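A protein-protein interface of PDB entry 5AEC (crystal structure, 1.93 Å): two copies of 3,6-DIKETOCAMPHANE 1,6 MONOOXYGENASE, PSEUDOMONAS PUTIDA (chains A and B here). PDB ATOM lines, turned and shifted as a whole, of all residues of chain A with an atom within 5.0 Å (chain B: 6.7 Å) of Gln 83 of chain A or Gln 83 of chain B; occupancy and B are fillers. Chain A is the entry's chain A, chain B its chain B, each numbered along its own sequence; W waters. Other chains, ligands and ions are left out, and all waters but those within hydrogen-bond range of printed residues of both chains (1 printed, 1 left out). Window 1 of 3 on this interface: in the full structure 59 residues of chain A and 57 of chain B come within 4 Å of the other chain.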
ATOM      1  N   GLU A  45     -10.283  -1.138 -23.827  1.00  0.00           N
ATOM      2  CA  GLU A  45     -10.730  -2.350 -23.118  1.00  0.00           C
ATOM      3  C   GLU A  45     -12.194  -2.192 -22.705  1.00  0.00           C
ATOM      4  O   GLU A  45     -12.532  -1.196 -22.062  1.00  0.00           O
ATOM      5  CB  GLU A  45      -9.916  -2.532 -21.838  1.00  0.00           C
ATOM      6  CG  GLU A  45     -10.280  -3.739 -20.968  1.00  0.00           C
ATOM      7  CD  GLU A  45      -9.277  -3.957 -19.860  1.00  0.00           C
ATOM      8  OE1 GLU A  45      -8.073  -4.180 -20.181  1.00  0.00           O
ATOM      9  OE2 GLU A  45      -9.678  -3.832 -18.673  1.00  0.00           O
ATOM     10  N   HIS A  78      -6.293  -0.344 -19.392  1.00  0.00           N
ATOM     11  CA  HIS A  78      -6.576  -1.426 -18.462  1.00  0.00           C
ATOM     12  C   HIS A  78      -7.433  -0.855 -17.326  1.00  0.00           C
ATOM     13  O   HIS A  78      -7.121   0.167 -16.732  1.00  0.00           O
ATOM     14  CB  HIS A  78      -5.302  -2.074 -17.897  1.00  0.00           C
ATOM     15  CG  HIS A  78      -4.616  -3.009 -18.841  1.00  0.00           C
ATOM     16  ND1 HIS A  78      -5.301  -3.886 -19.658  1.00  0.00           N
ATOM     17  CD2 HIS A  78      -3.300  -3.227 -19.075  1.00  0.00           C
ATOM     18  CE1 HIS A  78      -4.432  -4.589 -20.362  1.00  0.00           C
ATOM     19  NE2 HIS A  78      -3.214  -4.211 -20.022  1.00  0.00           N
ATOM     20  N   LEU A  79      -8.541  -1.517 -17.058  1.00  0.00           N
ATOM     21  CA  LEU A  79      -9.480  -1.099 -16.034  1.00  0.00           C
ATOM     22  C   LEU A  79      -9.071  -1.817 -14.772  1.00  0.00           C
ATOM     23  O   LEU A  79      -9.354  -3.023 -14.574  1.00  0.00           O
ATOM     24  CB  LEU A  79     -10.943  -1.425 -16.447  1.00  0.00           C
ATOM     25  CG  LEU A  79     -11.300  -0.855 -17.833  1.00  0.00           C
ATOM     26  CD1 LEU A  79     -12.761  -1.136 -18.175  1.00  0.00           C
ATOM     27  CD2 LEU A  79     -11.031   0.646 -17.900  1.00  0.00           C
ATOM     28  N   LEU A  80      -8.349  -1.066 -13.934  1.00  0.00           N
ATOM     29  CA  LEU A  80      -7.701  -1.635 -12.783  1.00  0.00           C
ATOM     30  C   LEU A  80      -8.667  -2.292 -11.756  1.00  0.00           C
ATOM     31  O   LEU A  80      -8.314  -3.311 -11.140  1.00  0.00           O
ATOM     32  CB  LEU A  80      -6.797  -0.615 -12.110  1.00  0.00           C
ATOM     33  CG  LEU A  80      -5.719   0.104 -12.934  1.00  0.00           C
ATOM     34  CD1 LEU A  80      -4.670   0.763 -12.038  1.00  0.00           C
ATOM     35  CD2 LEU A  80      -5.066  -0.829 -13.913  1.00  0.00           C
ATOM     36  N   PRO A  81      -9.909  -1.780 -11.640  1.00  0.00           N
ATOM     37  CA  PRO A  81     -10.854  -2.462 -10.709  1.00  0.00           C
ATOM     38  C   PRO A  81     -11.289  -3.863 -11.123  1.00  0.00           C
ATOM     39  O   PRO A  81     -11.910  -4.540 -10.326  1.00  0.00           O
ATOM     40  CB  PRO A  81     -12.075  -1.528 -10.695  1.00  0.00           C
ATOM     41  CG  PRO A  81     -11.491  -0.182 -10.988  1.00  0.00           C
ATOM     42  CD  PRO A  81     -10.418  -0.453 -12.031  1.00  0.00           C
ATOM     43  N   HIS A  82     -11.019  -4.273 -12.374  1.00  0.00           N
ATOM     44  CA  HIS A  82     -11.525  -5.517 -12.900  1.00  0.00           C
ATOM     45  C   HIS A  82     -10.588  -6.683 -12.812  1.00  0.00           C
ATOM     46  O   HIS A  82     -10.954  -7.773 -13.262  1.00  0.00           O
ATOM     47  CB  HIS A  82     -11.917  -5.341 -14.350  1.00  0.00           C
ATOM     48  CG  HIS A  82     -13.037  -4.387 -14.573  1.00  0.00           C
ATOM     49  ND1 HIS A  82     -13.539  -4.144 -15.830  1.00  0.00           N
ATOM     50  CD2 HIS A  82     -13.757  -3.615 -13.721  1.00  0.00           C
ATOM     51  CE1 HIS A  82     -14.523  -3.267 -15.746  1.00  0.00           C
ATOM     52  NE2 HIS A  82     -14.688  -2.944 -14.477  1.00  0.00           N
ATOM     53  N   GLN A  83      -9.365  -6.518 -12.306  1.00  0.00           N
ATOM     54  CA  GLN A  83      -8.473  -7.672 -12.216  1.00  0.00           C
ATOM     55  C   GLN A  83      -7.550  -7.601 -11.023  1.00  0.00           C
ATOM     56  O   GLN A  83      -7.394  -6.567 -10.402  1.00  0.00           O
ATOM     57  CB  GLN A  83      -7.701  -7.904 -13.534  1.00  0.00           C
ATOM     58  CG  GLN A  83      -7.159  -6.702 -14.270  1.00  0.00           C
ATOM     59  CD  GLN A  83      -6.453  -7.146 -15.533  1.00  0.00           C
ATOM     60  OE1 GLN A  83      -6.629  -6.567 -16.605  1.00  0.00           O
ATOM     61  NE2 GLN A  83      -5.671  -8.215 -15.416  1.00  0.00           N
ATOM     62  N   HIS A  84      -6.981  -8.750 -10.678  1.00  0.00           N
ATOM     63  CA  HIS A  84      -6.066  -8.794  -9.573  1.00  0.00           C
ATOM     64  C   HIS A  84      -4.794  -8.015  -9.964  1.00  0.00           C
ATOM     65  O   HIS A  84      -4.219  -8.272 -11.025  1.00  0.00           O
ATOM     66  CB  HIS A  84      -5.730 -10.222  -9.160  1.00  0.00           C
ATOM     67  CG  HIS A  84      -5.095 -10.299  -7.804  1.00  0.00           C
ATOM     68  ND1 HIS A  84      -3.763 -10.044  -7.608  1.00  0.00           N
ATOM     69  CD2 HIS A  84      -5.623 -10.520  -6.574  1.00  0.00           C
ATOM     70  CE1 HIS A  84      -3.486 -10.124  -6.320  1.00  0.00           C
ATOM     71  NE2 HIS A  84      -4.601 -10.421  -5.672  1.00  0.00           N
ATOM     72  N   PRO A  85      -4.366  -7.069  -9.114  1.00  0.00           N
ATOM     73  CA  PRO A  85      -3.209  -6.248  -9.490  1.00  0.00           C
ATOM     74  C   PRO A  85      -1.879  -7.014  -9.680  1.00  0.00           C
ATOM     75  O   PRO A  85      -1.029  -6.575 -10.450  1.00  0.00           O
ATOM     76  CB  PRO A  85      -3.097  -5.218  -8.359  1.00  0.00           C
ATOM     77  CG  PRO A  85      -4.373  -5.280  -7.614  1.00  0.00           C
ATOM     78  CD  PRO A  85      -4.944  -6.651  -7.813  1.00  0.00           C
ATOM     79  N   LYS A  87      -1.545 -10.160 -10.906  1.00  0.00           N
ATOM     80  CA  LYS A  87      -1.695 -10.813 -12.190  1.00  0.00           C
ATOM     81  C   LYS A  87      -1.501  -9.811 -13.312  1.00  0.00           C
ATOM     82  O   LYS A  87      -0.800 -10.087 -14.288  1.00  0.00           O
ATOM     83  CB  LYS A  87      -3.080 -11.456 -12.304  1.00  0.00           C
ATOM     84  CG  LYS A  87      -3.228 -12.431 -13.458  1.00  0.00           C
ATOM     85  CD  LYS A  87      -2.480 -13.712 -13.152  1.00  0.00           C
ATOM     86  CE  LYS A  87      -2.610 -14.718 -14.264  1.00  0.00           C
ATOM     87  NZ  LYS A  87      -2.115 -14.202 -15.552  1.00  0.00           N
ATOM     88  N   LEU A  88      -2.116  -8.641 -13.160  1.00  0.00           N
ATOM     89  CA  LEU A  88      -1.984  -7.577 -14.137  1.00  0.00           C
ATOM     90  C   LEU A  88      -0.561  -7.045 -14.221  1.00  0.00           C
ATOM     91  O   LEU A  88      -0.012  -6.858 -15.335  1.00  0.00           O
ATOM     92  CB  LEU A  88      -2.953  -6.453 -13.787  1.00  0.00           C
ATOM     93  CG  LEU A  88      -2.982  -5.252 -14.716  1.00  0.00           C
ATOM     94  CD1 LEU A  88      -3.084  -5.629 -16.181  1.00  0.00           C
ATOM     95  CD2 LEU A  88      -4.159  -4.369 -14.336  1.00  0.00           C
ATOM     96  N   TRP A 166      -7.839  -5.861  -2.443  1.00  0.00           N
ATOM     97  CA  TRP A 166      -7.063  -7.064  -2.768  1.00  0.00           C
ATOM     98  C   TRP A 166      -5.981  -7.307  -1.750  1.00  0.00           C
ATOM     99  O   TRP A 166      -5.543  -6.374  -1.064  1.00  0.00           O
ATOM    100  CB  TRP A 166      -6.340  -6.916  -4.113  1.00  0.00           C
ATOM    101  CG  TRP A 166      -7.193  -6.645  -5.295  1.00  0.00           C
ATOM    102  CD1 TRP A 166      -7.846  -7.566  -6.072  1.00  0.00           C
ATOM    103  CD2 TRP A 166      -7.434  -5.374  -5.897  1.00  0.00           C
ATOM    104  NE1 TRP A 166      -8.477  -6.945  -7.101  1.00  0.00           N
ATOM    105  CE2 TRP A 166      -8.248  -5.596  -7.024  1.00  0.00           C
ATOM    106  CE3 TRP A 166      -7.027  -4.065  -5.600  1.00  0.00           C
ATOM    107  CZ2 TRP A 166      -8.682  -4.554  -7.853  1.00  0.00           C
ATOM    108  CZ3 TRP A 166      -7.455  -3.028  -6.418  1.00  0.00           C
ATOM    109  CH2 TRP A 166      -8.273  -3.278  -7.544  1.00  0.00           C
ATOM    110  N   LEU B  79      -4.401 -20.565 -13.538  1.00  0.00           N
ATOM    111  CA  LEU B  79      -4.458 -20.726 -12.080  1.00  0.00           C
ATOM    112  C   LEU B  79      -5.574 -19.829 -11.581  1.00  0.00           C
ATOM    113  O   LEU B  79      -5.446 -18.575 -11.499  1.00  0.00           O
ATOM    114  CB  LEU B  79      -3.114 -20.398 -11.458  1.00  0.00           C
ATOM    115  CG  LEU B  79      -1.963 -21.179 -12.109  1.00  0.00           C
ATOM    116  CD1 LEU B  79      -0.621 -20.876 -11.412  1.00  0.00           C
ATOM    117  CD2 LEU B  79      -2.227 -22.673 -12.086  1.00  0.00           C
ATOM    118  N   LEU B  80      -6.702 -20.463 -11.289  1.00  0.00           N
ATOM    119  CA  LEU B  80      -7.934 -19.740 -10.980  1.00  0.00           C
ATOM    120  C   LEU B  80      -7.858 -18.847  -9.736  1.00  0.00           C
ATOM    121  O   LEU B  80      -8.492 -17.771  -9.706  1.00  0.00           O
ATOM    122  CB  LEU B  80      -9.128 -20.703 -10.910  1.00  0.00           C
ATOM    123  CG  LEU B  80      -9.395 -21.605 -12.129  1.00  0.00           C
ATOM    124  CD1 LEU B  80     -10.828 -22.156 -12.075  1.00  0.00           C
ATOM    125  CD2 LEU B  80      -9.161 -20.889 -13.433  1.00  0.00           C
ATOM    126  N   PRO B  81      -7.035 -19.230  -8.741  1.00  0.00           N
ATOM    127  CA  PRO B  81      -6.946 -18.361  -7.578  1.00  0.00           C
ATOM    128  C   PRO B  81      -6.251 -17.023  -7.824  1.00  0.00           C
ATOM    129  O   PRO B  81      -6.317 -16.166  -6.964  1.00  0.00           O
ATOM    130  CB  PRO B  81      -6.137 -19.193  -6.576  1.00  0.00           C
ATOM    131  CG  PRO B  81      -6.452 -20.599  -6.925  1.00  0.00           C
ATOM    132  CD  PRO B  81      -6.522 -20.583  -8.433  1.00  0.00           C
ATOM    133  N   HIS B  82      -5.615 -16.857  -8.977  1.00  0.00           N
ATOM    134  CA  HIS B  82      -4.797 -15.686  -9.254  1.00  0.00           C
ATOM    135  C   HIS B  82      -5.466 -14.592 -10.043  1.00  0.00           C
ATOM    136  O   HIS B  82      -4.819 -13.570 -10.298  1.00  0.00           O
ATOM    137  CB  HIS B  82      -3.543 -16.110 -10.025  1.00  0.00           C
ATOM    138  CG  HIS B  82      -2.632 -17.011  -9.264  1.00  0.00           C
ATOM    139  ND1 HIS B  82      -1.438 -17.447  -9.785  1.00  0.00           N
ATOM    140  CD2 HIS B  82      -2.728 -17.547  -8.028  1.00  0.00           C
ATOM    141  CE1 HIS B  82      -0.835 -18.219  -8.904  1.00  0.00           C
ATOM    142  NE2 HIS B  82      -1.602 -18.305  -7.830  1.00  0.00           N
ATOM    143  N   GLN B  83      -6.728 -14.759 -10.459  1.00  0.00           N
ATOM    144  CA  GLN B  83      -7.400 -13.739 -11.260  1.00  0.00           C
ATOM    145  C   GLN B  83      -8.885 -13.622 -10.919  1.00  0.00           C
ATOM    146  O   GLN B  83      -9.459 -14.533 -10.394  1.00  0.00           O
ATOM    147  CB  GLN B  83      -7.211 -14.082 -12.738  1.00  0.00           C
ATOM    148  CG  GLN B  83      -7.828 -13.135 -13.742  1.00  0.00           C
ATOM    149  CD  GLN B  83      -7.355 -11.679 -13.635  1.00  0.00           C
ATOM    150  OE1 GLN B  83      -7.295 -11.098 -12.556  1.00  0.00           O
ATOM    151  NE2 GLN B  83      -7.056 -11.079 -14.787  1.00  0.00           N
ATOM    152  N   HIS B  84      -9.469 -12.477 -11.217  1.00  0.00           N
ATOM    153  CA  HIS B  84     -10.894 -12.303 -11.061  1.00  0.00           C
ATOM    154  C   HIS B  84     -11.622 -13.199 -12.074  1.00  0.00           C
ATOM    155  O   HIS B  84     -11.265 -13.188 -13.261  1.00  0.00           O
ATOM    156  CB  HIS B  84     -11.301 -10.860 -11.259  1.00  0.00           C
ATOM    157  CG  HIS B  84     -12.671 -10.581 -10.736  1.00  0.00           C
ATOM    158  ND1 HIS B  84     -13.794 -10.877 -11.455  1.00  0.00           N
ATOM    159  CD2 HIS B  84     -13.102 -10.124  -9.533  1.00  0.00           C
ATOM    160  CE1 HIS B  84     -14.869 -10.562 -10.750  1.00  0.00           C
ATOM    161  NE2 HIS B  84     -14.476 -10.119  -9.572  1.00  0.00           N
ATOM    162  N   PRO B  85     -12.580 -14.027 -11.605  1.00  0.00           N
ATOM    163  CA  PRO B  85     -13.195 -14.992 -12.504  1.00  0.00           C
ATOM    164  C   PRO B  85     -13.968 -14.384 -13.657  1.00  0.00           C
ATOM    165  O   PRO B  85     -14.065 -15.007 -14.707  1.00  0.00           O
ATOM    166  CB  PRO B  85     -14.105 -15.808 -11.590  1.00  0.00           C
ATOM    167  CG  PRO B  85     -13.660 -15.518 -10.179  1.00  0.00           C
ATOM    168  CD  PRO B  85     -13.014 -14.190 -10.192  1.00  0.00           C
ATOM    169  N   ALA B  86     -14.580 -13.221 -13.459  1.00  0.00           N
ATOM    170  CA  ALA B  86     -15.243 -12.521 -14.575  1.00  0.00           C
ATOM    171  C   ALA B  86     -14.296 -12.080 -15.681  1.00  0.00           C
ATOM    172  O   ALA B  86     -14.608 -12.211 -16.857  1.00  0.00           O
ATOM    173  CB  ALA B  86     -16.061 -11.326 -14.087  1.00  0.00           C
ATOM    174  N   LYS B  87     -13.151 -11.554 -15.280  1.00  0.00           N
ATOM    175  CA  LYS B  87     -12.131 -11.099 -16.218  1.00  0.00           C
ATOM    176  C   LYS B  87     -11.577 -12.267 -16.986  1.00  0.00           C
ATOM    177  O   LYS B  87     -11.438 -12.215 -18.228  1.00  0.00           O
ATOM    178  CB  LYS B  87     -11.013 -10.380 -15.477  1.00  0.00           C
ATOM    179  CG  LYS B  87     -10.054  -9.613 -16.380  1.00  0.00           C
ATOM    180  CD  LYS B  87     -10.713  -8.338 -16.869  1.00  0.00           C
ATOM    181  CE  LYS B  87      -9.791  -7.537 -17.745  1.00  0.00           C
ATOM    182  NZ  LYS B  87      -9.328  -8.308 -18.913  1.00  0.00           N
ATOM    183  N   LEU B  88     -11.293 -13.335 -16.270  1.00  0.00           N
ATOM    184  CA  LEU B  88     -10.806 -14.572 -16.879  1.00  0.00           C
ATOM    185  C   LEU B  88     -11.811 -15.238 -17.809  1.00  0.00           C
ATOM    186  O   LEU B  88     -11.484 -15.609 -18.949  1.00  0.00           O
ATOM    187  CB  LEU B  88     -10.391 -15.531 -15.788  1.00  0.00           C
ATOM    188  CG  LEU B  88      -9.820 -16.878 -16.213  1.00  0.00           C
ATOM    189  CD1 LEU B  88      -8.733 -16.727 -17.289  1.00  0.00           C
ATOM    190  CD2 LEU B  88      -9.299 -17.576 -14.999  1.00  0.00           C
ATOM    191  N   HIS B 119      -0.154 -13.424  -5.322  1.00  0.00           N
ATOM    192  CA  HIS B 119      -1.578 -13.186  -5.585  1.00  0.00           C
ATOM    193  C   HIS B 119      -2.440 -13.170  -4.333  1.00  0.00           C
ATOM    194  O   HIS B 119      -3.663 -13.225  -4.433  1.00  0.00           O
ATOM    195  CB  HIS B 119      -2.089 -14.206  -6.589  1.00  0.00           C
ATOM    196  CG  HIS B 119      -1.391 -14.106  -7.907  1.00  0.00           C
ATOM    197  ND1 HIS B 119      -0.228 -14.793  -8.191  1.00  0.00           N
ATOM    198  CD2 HIS B 119      -1.650 -13.344  -8.990  1.00  0.00           C
ATOM    199  CE1 HIS B 119       0.178 -14.498  -9.413  1.00  0.00           C
ATOM    200  NE2 HIS B 119      -0.666 -13.620  -9.920  1.00  0.00           N
ATOM    201  N   SER B 146     -14.305 -19.981  -8.435  1.00  0.00           N
ATOM    202  CA  SER B 146     -14.034 -19.374  -9.743  1.00  0.00           C
ATOM    203  C   SER B 146     -14.813 -20.093 -10.846  1.00  0.00           C
ATOM    204  O   SER B 146     -15.462 -19.453 -11.652  1.00  0.00           O
ATOM    205  CB  SER B 146     -12.523 -19.369 -10.042  1.00  0.00           C
ATOM    206  OG  SER B 146     -12.285 -18.998 -11.400  1.00  0.00           O
ATOM    207  N   TRP B 166     -14.546 -13.807  -4.264  1.00  0.00           N
ATOM    208  CA  TRP B 166     -14.825 -12.743  -5.226  1.00  0.00           C
ATOM    209  C   TRP B 166     -16.303 -12.379  -5.249  1.00  0.00           C
ATOM    210  O   TRP B 166     -17.160 -13.209  -4.896  1.00  0.00           O
ATOM    211  CB  TRP B 166     -14.480 -13.180  -6.650  1.00  0.00           C
ATOM    212  CG  TRP B 166     -13.063 -13.582  -6.884  1.00  0.00           C
ATOM    213  CD1 TRP B 166     -12.009 -12.760  -7.150  1.00  0.00           C
ATOM    214  CD2 TRP B 166     -12.574 -14.906  -6.958  1.00  0.00           C
ATOM    215  NE1 TRP B 166     -10.877 -13.495  -7.337  1.00  0.00           N
ATOM    216  CE2 TRP B 166     -11.182 -14.821  -7.233  1.00  0.00           C
ATOM    217  CE3 TRP B 166     -13.157 -16.161  -6.777  1.00  0.00           C
ATOM    218  CZ2 TRP B 166     -10.370 -15.944  -7.349  1.00  0.00           C
ATOM    219  CZ3 TRP B 166     -12.355 -17.291  -6.885  1.00  0.00           C
ATOM    220  CH2 TRP B 166     -10.967 -17.182  -7.184  1.00  0.00           C
HETATM  221  O   HOH W   1      -7.298  -6.676 -20.190  1.00  0.00           O
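The side-chain amide nitrogen (NE2) of Gln 83 of chain A sits close to the side-chain amide nitrogen (NE2) of Gln 83 of chain B (3.2 Å). The side-chain amide oxygen (OE1) of Gln 83 of chain B lies within hydrogen-bond range of the backbone NH (N) of His 84 of chain A, at 3.0 Å. A ring nitrogen (NE2) of His 84 of chain A lies within hydrogen-bond range of the backbone carbonyl oxygen (O) of His 119 of chain B, at 3.2 Å.
Of the printed residues of chain B, Gln 83 of chain A touches Gln 83 (3.2 Å) and Lys 87 (3.5 Å). Printed residues of chain B within 4 Å of Lys 87 of chain A: His 82 and His 119. Printed residues of chain A within 4 Å of His 82 of chain B: His 84 and Lys 87. Of the printed residues of chain A, Gln 83 of chain B touches Gln 83 and His 84. Of the printed residues of chain A, His 84 of chain B touches His 82. Of the printed residues of chain A, Lys 87 of chain B touches Glu 45 (3.8 Å), His 82 (3.4 Å) and Gln 83 (3.5 Å). Of the printed residues of chain A, His 119 of chain B touches His 84 and Lys 87. The nearest printed residue of chain B that does not touch Gln 83 of chain A is His 84 of chain B (4.4 Å). The nearest printed residue of chain A that does not touch Gln 83 of chain B is Lys 87 of chain A (4.2 Å).
Water W1 lies within hydrogen-bond range of the side-chain carboxylate of Glu 45 of chain A, the side-chain amino group of Lys 87 of chain B and a ring nitrogen (ND1) of His 78 of chain A.
His 82 of chain A touches His 84 of chain B, and with the chains exchanged His 84 of chain A touches His 82 of chain B. His 82 of chain A touches Lys 87 of chain B, and with the chains exchanged Lys 87 of chain A touches His 82 of chain B. Gln 83 of chain A touches Lys 87 of chain B, but with the chains exchanged Lys 87 of chain A does not touch Gln 83 of chain B (4.2 Å). His 84 of chain A touches Gln 83 of chain B, but with the chains exchanged Gln 83 of chain A does not touch His 84 of chain B (4.4 Å). Positions printed for both chains: 79, 80, 81, 82, 83, 84, 85, 87, 88 and 166.
The side-chain carboxylate of Glu 45 of chain A is in hydrogen-bond range of a ring nitrogen (ND1) of His 78 of chain A. The side-chain carboxylate of Glu 45 of chain A is in hydrogen-bond range of the backbone NH of Leu 79 of chain A (3.0 Å). The backbone carbonyl oxygen of Gln 83 of chain A sits close to the indole nitrogen of Trp 166 of chain A. ND1 of His 82 of chain B sits at hydrogen-bond distance from ND1 of His 119 of chain B (3.3 Å). The backbone NH (N) of Ala 86 of chain B sits at hydrogen-bond distance from a ring nitrogen (ND1) of His 84 of chain B (3.2 Å).
Glu 45 of chain A touches Lys 87 of chain B (OE2 to CE, 3.8 Å). His 82 of chain A touches His 84 of chain B. His 82 of chain A touches Lys 87 of chain B (O to CB, 3.4 Å). Lys 87 of chain B touches Gln 83 of chain A. CB of His 84 of chain A touches O of His 82 of chain B (3.7 Å). Lys 87 of chain A touches His 82 of chain B. His 119 of chain B touches Lys 87 of chain A (NE2 to N, 3.7 Å).
Hydrophobic or aromatic side chains of chain B that line the printed part of chain A: His 84 and His 119. Hydrophobic or aromatic side chains of chain A that line the printed part of chain B: His 84. Among the printed residues, no Asp or Glu carboxylate lies within 4 Å of a Lys or Arg side-chain nitrogen of the other chain.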
